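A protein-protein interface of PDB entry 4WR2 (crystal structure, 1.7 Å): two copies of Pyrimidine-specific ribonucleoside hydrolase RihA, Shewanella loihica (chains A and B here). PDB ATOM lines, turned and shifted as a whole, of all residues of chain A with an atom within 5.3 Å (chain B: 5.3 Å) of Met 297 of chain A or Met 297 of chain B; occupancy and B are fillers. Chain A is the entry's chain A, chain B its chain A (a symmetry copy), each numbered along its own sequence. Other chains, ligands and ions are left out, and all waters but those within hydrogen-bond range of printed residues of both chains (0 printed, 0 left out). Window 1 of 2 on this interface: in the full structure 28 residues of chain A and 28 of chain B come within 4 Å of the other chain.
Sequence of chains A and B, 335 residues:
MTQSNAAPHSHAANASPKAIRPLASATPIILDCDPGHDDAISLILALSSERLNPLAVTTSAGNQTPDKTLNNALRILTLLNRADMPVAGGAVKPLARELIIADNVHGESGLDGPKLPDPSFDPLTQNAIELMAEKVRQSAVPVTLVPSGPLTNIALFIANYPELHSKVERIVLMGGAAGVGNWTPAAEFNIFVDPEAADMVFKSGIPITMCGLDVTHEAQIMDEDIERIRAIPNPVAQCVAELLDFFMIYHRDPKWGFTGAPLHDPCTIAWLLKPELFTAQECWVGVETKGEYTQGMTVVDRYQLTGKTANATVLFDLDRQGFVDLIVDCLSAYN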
ATOM      1  N   ALA A 177     -21.805 -19.703  20.449  1.00  0.00           N
ATOM      2  CA  ALA A 177     -21.621 -20.561  21.597  1.00  0.00           C
ATOM      3  C   ALA A 177     -20.782 -21.741  21.162  1.00  0.00           C
ATOM      4  O   ALA A 177     -21.074 -22.362  20.132  1.00  0.00           O
ATOM      5  CB  ALA A 177     -22.953 -21.045  22.161  1.00  0.00           C
ATOM      6  N   GLY A 179     -20.665 -24.763  21.466  1.00  0.00           N
ATOM      7  CA  GLY A 179     -21.298 -26.059  21.560  1.00  0.00           C
ATOM      8  C   GLY A 179     -22.767 -26.130  21.917  1.00  0.00           C
ATOM      9  O   GLY A 179     -23.467 -27.032  21.457  1.00  0.00           O
ATOM     10  N   ALA A 186     -28.134 -26.095  18.966  1.00  0.00           N
ATOM     11  CA  ALA A 186     -26.793 -25.836  18.433  1.00  0.00           C
ATOM     12  C   ALA A 186     -26.433 -24.377  18.277  1.00  0.00           C
ATOM     13  O   ALA A 186     -25.260 -24.063  18.132  1.00  0.00           O
ATOM     14  CB  ALA A 186     -26.653 -26.517  17.059  1.00  0.00           C
ATOM     15  N   ALA A 187     -27.432 -23.483  18.256  1.00  0.00           N
ATOM     16  CA  ALA A 187     -27.213 -22.092  17.878  1.00  0.00           C
ATOM     17  C   ALA A 187     -27.676 -21.057  18.870  1.00  0.00           C
ATOM     18  O   ALA A 187     -28.753 -21.176  19.460  1.00  0.00           O
ATOM     19  CB  ALA A 187     -27.933 -21.808  16.542  1.00  0.00           C
ATOM     20  N   ILE A 191     -26.517 -15.299  15.951  1.00  0.00           N
ATOM     21  CA  ILE A 191     -25.976 -16.020  14.801  1.00  0.00           C
ATOM     22  C   ILE A 191     -27.112 -16.696  14.049  1.00  0.00           C
ATOM     23  O   ILE A 191     -27.156 -16.643  12.810  1.00  0.00           O
ATOM     24  CB  ILE A 191     -24.902 -17.049  15.202  1.00  0.00           C
ATOM     25  CG1 ILE A 191     -23.848 -16.430  16.115  1.00  0.00           C
ATOM     26  CG2 ILE A 191     -24.237 -17.633  13.967  1.00  0.00           C
ATOM     27  CD1 ILE A 191     -23.091 -15.238  15.542  1.00  0.00           C
ATOM     28  N   GLY A 286     -16.006 -21.695  12.607  1.00  0.00           N
ATOM     29  CA  GLY A 286     -16.787 -21.745  11.386  1.00  0.00           C
ATOM     30  C   GLY A 286     -18.265 -21.584  11.723  1.00  0.00           C
ATOM     31  O   GLY A 286     -18.718 -22.054  12.746  1.00  0.00           O
ATOM     32  N   VAL A 287     -19.004 -20.898  10.863  1.00  0.00           N
ATOM     33  CA  VAL A 287     -20.450 -20.762  11.044  1.00  0.00           C
ATOM     34  C   VAL A 287     -21.162 -21.727  10.088  1.00  0.00           C
ATOM     35  O   VAL A 287     -20.962 -21.701   8.857  1.00  0.00           O
ATOM     36  CB  VAL A 287     -20.922 -19.337  10.755  1.00  0.00           C
ATOM     37  CG1 VAL A 287     -22.432 -19.262  10.911  1.00  0.00           C
ATOM     38  CG2 VAL A 287     -20.258 -18.353  11.703  1.00  0.00           C
ATOM     39  N   GLU A 288     -22.035 -22.552  10.654  1.00  0.00           N
ATOM     40  CA  GLU A 288     -22.776 -23.534   9.882  1.00  0.00           C
ATOM     41  C   GLU A 288     -23.971 -22.880   9.221  1.00  0.00           C
ATOM     42  O   GLU A 288     -24.813 -22.283   9.910  1.00  0.00           O
ATOM     43  CB  GLU A 288     -23.255 -24.671  10.786  1.00  0.00           C
ATOM     44  CG  GLU A 288     -24.028 -25.756  10.051  1.00  0.00           C
ATOM     45  CD  GLU A 288     -23.164 -26.436   9.021  1.00  0.00           C
ATOM     46  OE1 GLU A 288     -22.095 -26.932   9.410  1.00  0.00           O
ATOM     47  OE2 GLU A 288     -23.551 -26.459   7.831  1.00  0.00           O
ATOM     48  N   THR A 294     -28.367 -27.817  12.419  1.00  0.00           N
ATOM     49  CA  THR A 294     -27.324 -27.008  12.988  1.00  0.00           C
ATOM     50  C   THR A 294     -27.093 -25.645  12.384  1.00  0.00           C
ATOM     51  O   THR A 294     -26.040 -25.036  12.590  1.00  0.00           O
ATOM     52  CB  THR A 294     -26.007 -27.801  12.877  1.00  0.00           C
ATOM     53  OG1 THR A 294     -25.851 -28.230  11.520  1.00  0.00           O
ATOM     54  CG2 THR A 294     -26.022 -29.031  13.771  1.00  0.00           C
ATOM     55  N   GLN A 295     -28.044 -25.131  11.621  1.00  0.00           N
ATOM     56  CA  GLN A 295     -27.829 -23.817  11.021  1.00  0.00           C
ATOM     57  C   GLN A 295     -27.733 -22.788  12.147  1.00  0.00           C
ATOM     58  O   GLN A 295     -28.459 -22.857  13.147  1.00  0.00           O
ATOM     59  CB  GLN A 295     -28.946 -23.465  10.010  1.00  0.00           C
ATOM     60  CG  GLN A 295     -28.772 -24.277   8.707  1.00  0.00           C
ATOM     61  CD  GLN A 295     -29.890 -24.078   7.718  1.00  0.00           C
ATOM     62  OE1 GLN A 295     -30.358 -22.950   7.516  1.00  0.00           O
ATOM     63  NE2 GLN A 295     -30.334 -25.170   7.089  1.00  0.00           N
ATOM     64  N   GLY A 296     -26.754 -21.915  11.996  1.00  0.00           N
ATOM     65  CA  GLY A 296     -26.481 -20.883  12.981  1.00  0.00           C
ATOM     66  C   GLY A 296     -25.486 -21.308  14.050  1.00  0.00           C
ATOM     67  O   GLY A 296     -25.135 -20.512  14.921  1.00  0.00           O
ATOM     68  N   MET A 297     -25.037 -22.561  14.024  1.00  0.00           N
ATOM     69  CA  MET A 297     -24.041 -22.947  15.008  1.00  0.00           C
ATOM     70  C   MET A 297     -22.683 -22.286  14.725  1.00  0.00           C
ATOM     71  O   MET A 297     -22.270 -22.194  13.570  1.00  0.00           O
ATOM     72  CB  MET A 297     -23.837 -24.461  15.001  1.00  0.00           C
ATOM     73  CG  MET A 297     -22.705 -24.918  15.923  1.00  0.00           C
ATOM     74  SD  MET A 297     -22.689 -26.895  16.087  1.00  0.00           S
ATOM     75  CE  MET A 297     -21.440 -26.977  17.602  1.00  0.00           C
ATOM     76  N   THR A 298     -21.996 -21.828  15.767  1.00  0.00           N
ATOM     77  CA  THR A 298     -20.571 -21.479  15.670  1.00  0.00           C
ATOM     78  C   THR A 298     -19.777 -22.733  16.093  1.00  0.00           C
ATOM     79  O   THR A 298     -19.877 -23.226  17.225  1.00  0.00           O
ATOM     80  CB  THR A 298     -20.150 -20.313  16.583  1.00  0.00           C
ATOM     81  OG1 THR A 298     -20.550 -20.580  17.938  1.00  0.00           O
ATOM     82  CG2 THR A 298     -20.758 -19.030  16.103  1.00  0.00           C
ATOM     83  N   VAL A 299     -19.009 -23.278  15.144  1.00  0.00           N
ATOM     84  CA  VAL A 299     -18.218 -24.475  15.363  1.00  0.00           C
ATOM     85  C   VAL A 299     -16.839 -24.003  15.793  1.00  0.00           C
ATOM     86  O   VAL A 299     -16.062 -23.540  14.963  1.00  0.00           O
ATOM     87  CB  VAL A 299     -18.151 -25.321  14.064  1.00  0.00           C
ATOM     88  CG1 VAL A 299     -17.372 -26.588  14.296  1.00  0.00           C
ATOM     89  CG2 VAL A 299     -19.565 -25.646  13.605  1.00  0.00           C
ATOM     90  N   ALA B 177     -22.152 -36.553  21.681  1.00  0.00           N
ATOM     91  CA  ALA B 177     -21.778 -35.552  22.652  1.00  0.00           C
ATOM     92  C   ALA B 177     -22.762 -34.409  22.540  1.00  0.00           C
ATOM     93  O   ALA B 177     -23.033 -33.933  21.431  1.00  0.00           O
ATOM     94  CB  ALA B 177     -20.358 -35.045  22.425  1.00  0.00           C
ATOM     95  N   GLY B 179     -22.814 -31.371  22.479  1.00  0.00           N
ATOM     96  CA  GLY B 179     -22.260 -30.094  22.087  1.00  0.00           C
ATOM     97  C   GLY B 179     -20.808 -30.028  21.665  1.00  0.00           C
ATOM     98  O   GLY B 179     -20.454 -29.215  20.811  1.00  0.00           O
ATOM     99  N   ALA B 186     -17.580 -30.612  16.493  1.00  0.00           N
ATOM    100  CA  ALA B 186     -19.000 -30.891  16.724  1.00  0.00           C
ATOM    101  C   ALA B 186     -19.342 -32.346  16.949  1.00  0.00           C
ATOM    102  O   ALA B 186     -20.424 -32.637  17.439  1.00  0.00           O
ATOM    103  CB  ALA B 186     -19.818 -30.385  15.522  1.00  0.00           C
ATOM    104  N   ALA B 187     -18.452 -33.268  16.554  1.00  0.00           N
ATOM    105  CA  ALA B 187     -18.782 -34.688  16.511  1.00  0.00           C
ATOM    106  C   ALA B 187     -17.858 -35.604  17.270  1.00  0.00           C
ATOM    107  O   ALA B 187     -16.636 -35.448  17.236  1.00  0.00           O
ATOM    108  CB  ALA B 187     -18.801 -35.161  15.041  1.00  0.00           C
ATOM    109  N   ILE B 191     -20.109 -41.642  16.046  1.00  0.00           N
ATOM    110  CA  ILE B 191     -21.167 -41.054  15.228  1.00  0.00           C
ATOM    111  C   ILE B 191     -20.569 -40.517  13.938  1.00  0.00           C
ATOM    112  O   ILE B 191     -21.137 -40.727  12.854  1.00  0.00           O
ATOM    113  CB  ILE B 191     -21.940 -39.948  15.972  1.00  0.00           C
ATOM    114  CG1 ILE B 191     -22.390 -40.412  17.354  1.00  0.00           C
ATOM    115  CG2 ILE B 191     -23.144 -39.503  15.159  1.00  0.00           C
ATOM    116  CD1 ILE B 191     -23.291 -41.641  17.381  1.00  0.00           C
ATOM    117  N   GLY B 286     -31.114 -35.373  17.509  1.00  0.00           N
ATOM    118  CA  GLY B 286     -31.034 -35.504  16.067  1.00  0.00           C
ATOM    119  C   GLY B 286     -29.577 -35.670  15.654  1.00  0.00           C
ATOM    120  O   GLY B 286     -28.696 -35.090  16.255  1.00  0.00           O
ATOM    121  N   VAL B 287     -29.331 -36.483  14.636  1.00  0.00           N
ATOM    122  CA  VAL B 287     -27.980 -36.643  14.101  1.00  0.00           C
ATOM    123  C   VAL B 287     -27.860 -35.830  12.805  1.00  0.00           C
ATOM    124  O   VAL B 287     -28.636 -36.005  11.845  1.00  0.00           O
ATOM    125  CB  VAL B 287     -27.662 -38.108  13.799  1.00  0.00           C
ATOM    126  CG1 VAL B 287     -26.269 -38.213  13.203  1.00  0.00           C
ATOM    127  CG2 VAL B 287     -27.744 -38.942  15.067  1.00  0.00           C
ATOM    128  N   GLU B 288     -26.849 -34.970  12.761  1.00  0.00           N
ATOM    129  CA  GLU B 288     -26.615 -34.118  11.609  1.00  0.00           C
ATOM    130  C   GLU B 288     -25.877 -34.890  10.535  1.00  0.00           C
ATOM    131  O   GLU B 288     -24.786 -35.423  10.792  1.00  0.00           O
ATOM    132  CB  GLU B 288     -25.792 -32.893  12.010  1.00  0.00           C
ATOM    133  CG  GLU B 288     -25.515 -31.935  10.861  1.00  0.00           C
ATOM    134  CD  GLU B 288     -26.795 -31.362  10.310  1.00  0.00           C
ATOM    135  OE1 GLU B 288     -27.552 -30.786  11.107  1.00  0.00           O
ATOM    136  OE2 GLU B 288     -27.042 -31.502   9.092  1.00  0.00           O
ATOM    137  N   THR B 294     -20.644 -29.738  10.516  1.00  0.00           N
ATOM    138  CA  THR B 294     -21.246 -30.433  11.620  1.00  0.00           C
ATOM    139  C   THR B 294     -21.699 -31.853  11.384  1.00  0.00           C
ATOM    140  O   THR B 294     -22.494 -32.396  12.155  1.00  0.00           O
ATOM    141  CB  THR B 294     -22.474 -29.617  12.070  1.00  0.00           C
ATOM    142  OG1 THR B 294     -23.289 -29.358  10.922  1.00  0.00           O
ATOM    143  CG2 THR B 294     -22.063 -28.286  12.678  1.00  0.00           C
ATOM    144  N   GLN B 295     -21.227 -32.490  10.324  1.00  0.00           N
ATOM    145  CA  GLN B 295     -21.665 -33.862  10.078  1.00  0.00           C
ATOM    146  C   GLN B 295     -21.163 -34.737  11.226  1.00  0.00           C
ATOM    147  O   GLN B 295     -20.042 -34.566  11.723  1.00  0.00           O
ATOM    148  CB  GLN B 295     -21.177 -34.375   8.702  1.00  0.00           C
ATOM    149  CG  GLN B 295     -21.994 -33.728   7.562  1.00  0.00           C
ATOM    150  CD  GLN B 295     -21.499 -34.088   6.186  1.00  0.00           C
ATOM    151  OE1 GLN B 295     -21.152 -35.247   5.925  1.00  0.00           O
ATOM    152  NE2 GLN B 295     -21.456 -33.099   5.289  1.00  0.00           N
ATOM    153  N   GLY B 296     -22.060 -35.589  11.686  1.00  0.00           N
ATOM    154  CA  GLY B 296     -21.781 -36.479  12.799  1.00  0.00           C
ATOM    155  C   GLY B 296     -22.137 -35.890  14.155  1.00  0.00           C
ATOM    156  O   GLY B 296     -21.990 -36.558  15.178  1.00  0.00           O
ATOM    157  N   MET B 297     -22.583 -34.636  14.195  1.00  0.00           N
ATOM    158  CA  MET B 297     -22.981 -34.096  15.483  1.00  0.00           C
ATOM    159  C   MET B 297     -24.280 -34.742  15.988  1.00  0.00           C
ATOM    160  O   MET B 297     -25.203 -34.965  15.206  1.00  0.00           O
ATOM    161  CB  MET B 297     -23.212 -32.589  15.386  1.00  0.00           C
ATOM    162  CG  MET B 297     -23.761 -31.983  16.679  1.00  0.00           C
ATOM    163  SD  MET B 297     -23.760 -30.001  16.579  1.00  0.00           S
ATOM    164  CE  MET B 297     -24.108 -29.687  18.488  1.00  0.00           C
ATOM    165  N   THR B 298     -24.352 -35.042  17.281  1.00  0.00           N
ATOM    166  CA  THR B 298     -25.630 -35.354  17.940  1.00  0.00           C
ATOM    167  C   THR B 298     -26.155 -34.030  18.537  1.00  0.00           C
ATOM    168  O   THR B 298     -25.530 -33.402  19.401  1.00  0.00           O
ATOM    169  CB  THR B 298     -25.510 -36.381  19.082  1.00  0.00           C
ATOM    170  OG1 THR B 298     -24.506 -35.959  20.020  1.00  0.00           O
ATOM    171  CG2 THR B 298     -25.173 -37.733  18.531  1.00  0.00           C
ATOM    172  N   VAL B 299     -27.308 -33.584  18.026  1.00  0.00           N
ATOM    173  CA  VAL B 299     -27.929 -32.343  18.452  1.00  0.00           C
ATOM    174  C   VAL B 299     -28.904 -32.711  19.558  1.00  0.00           C
ATOM    175  O   VAL B 299     -29.971 -33.249  19.281  1.00  0.00           O
ATOM    176  CB  VAL B 299     -28.652 -31.666  17.258  1.00  0.00           C
ATOM    177  CG1 VAL B 299     -29.259 -30.355  17.680  1.00  0.00           C
ATOM    178  CG2 VAL B 299     -27.656 -31.448  16.127  1.00  0.00           C
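OE1 of Glu 288 of chain A lies within hydrogen-bond range of OG1 of Thr 294 of chain B. The side-chain hydroxyl (OG1) of Thr 294 of chain A lies within hydrogen-bond range of the side-chain carboxylate (OE1) of Glu 288 of chain B. The side-chain hydroxyl (OG1) of Thr 294 of chain A lies within hydrogen-bond range of the side-chain hydroxyl (OG1) of Thr 294 of chain B (2.9 Å). SD of Met 297 of chain A sits close to SD of Met 297 of chain B (3.3 Å).
The backbone carbonyl oxygen (O) of Gly 286 of chain A lies within hydrogen-bond range of the backbone NH (N) of Val 299 of chain A (2.7 Å). O of Glu 288 of chain A is in hydrogen-bond range of N of Gly 296 of chain A. The backbone NH (N) of Glu 288 of chain A is in hydrogen-bond range of the backbone carbonyl oxygen (O) of Met 297 of chain A. The backbone carbonyl oxygen (O) of Gly 286 of chain B sits at hydrogen-bond distance from the backbone NH (N) of Val 299 of chain B (2.7 Å). The backbone NH (N) of Gly 296 of chain B sits at hydrogen-bond distance from the backbone carbonyl oxygen (O) of Glu 288 of chain B (2.9 Å). The backbone NH (N) of Glu 288 of chain B sits at hydrogen-bond distance from the backbone carbonyl oxygen (O) of Met 297 of chain B (2.9 Å).
Among the printed residues, pairs that only touch across the chains: Gly 179 of chain A with Gly 179 of chain B, Thr 294 of chain A with Met 297 of chain B, Met 297 of chain A with Thr 294 of chain B, Thr 294 of chain A with Val 299 of chain B and Val 299 of chain A with Thr 294 of chain B.
Of chain A, only Thr 294 (3.7 Å) and Met 297 (3.3 Å) come within 4 Å of Met 297 of chain B. Printed residues of chain B within 4 Å of Thr 294 of chain A: Glu 288 (3.1 Å), Thr 294 (2.9 Å), Met 297 (3.7 Å) and Val 299 (3.8 Å). Of the printed residues of chain A, Thr 294 of chain B touches Glu 288, Thr 294, Met 297 and Val 299. Gln 295 of chain B touches none of the printed residues of chain A. The nearest printed residue of chain A that does not touch Gly 179 of chain B is Met 297 of chain A (4.03 Å).
Hydrophobic or aromatic side chains of chain B that line the printed part of chain A: Met 297 and Val 299. Among the printed residues, no Asp or Glu carboxylate lies within 4 Å of a Lys or Arg side-chain nitrogen of the other chain.
Gly 179 of chain A touches its own counterpart, Gly 179 of chain B. Glu 288 of chain A touches Thr 294 of chain B, and with the chains exchanged Thr 294 of chain A touches Glu 288 of chain B. Thr 294 of chain A touches Met 297 of chain B, and with the chains exchanged Met 297 of chain A touches Thr 294 of chain B. Thr 294 of chain A touches Val 299 of chain B, and with the chains exchanged Val 299 of chain A touches Thr 294 of chain B. 14 positions are printed for both chains. Of the 9 pairs that touch across the chains among the printed residues, 9 have their exchanged pair printed and touching as well.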
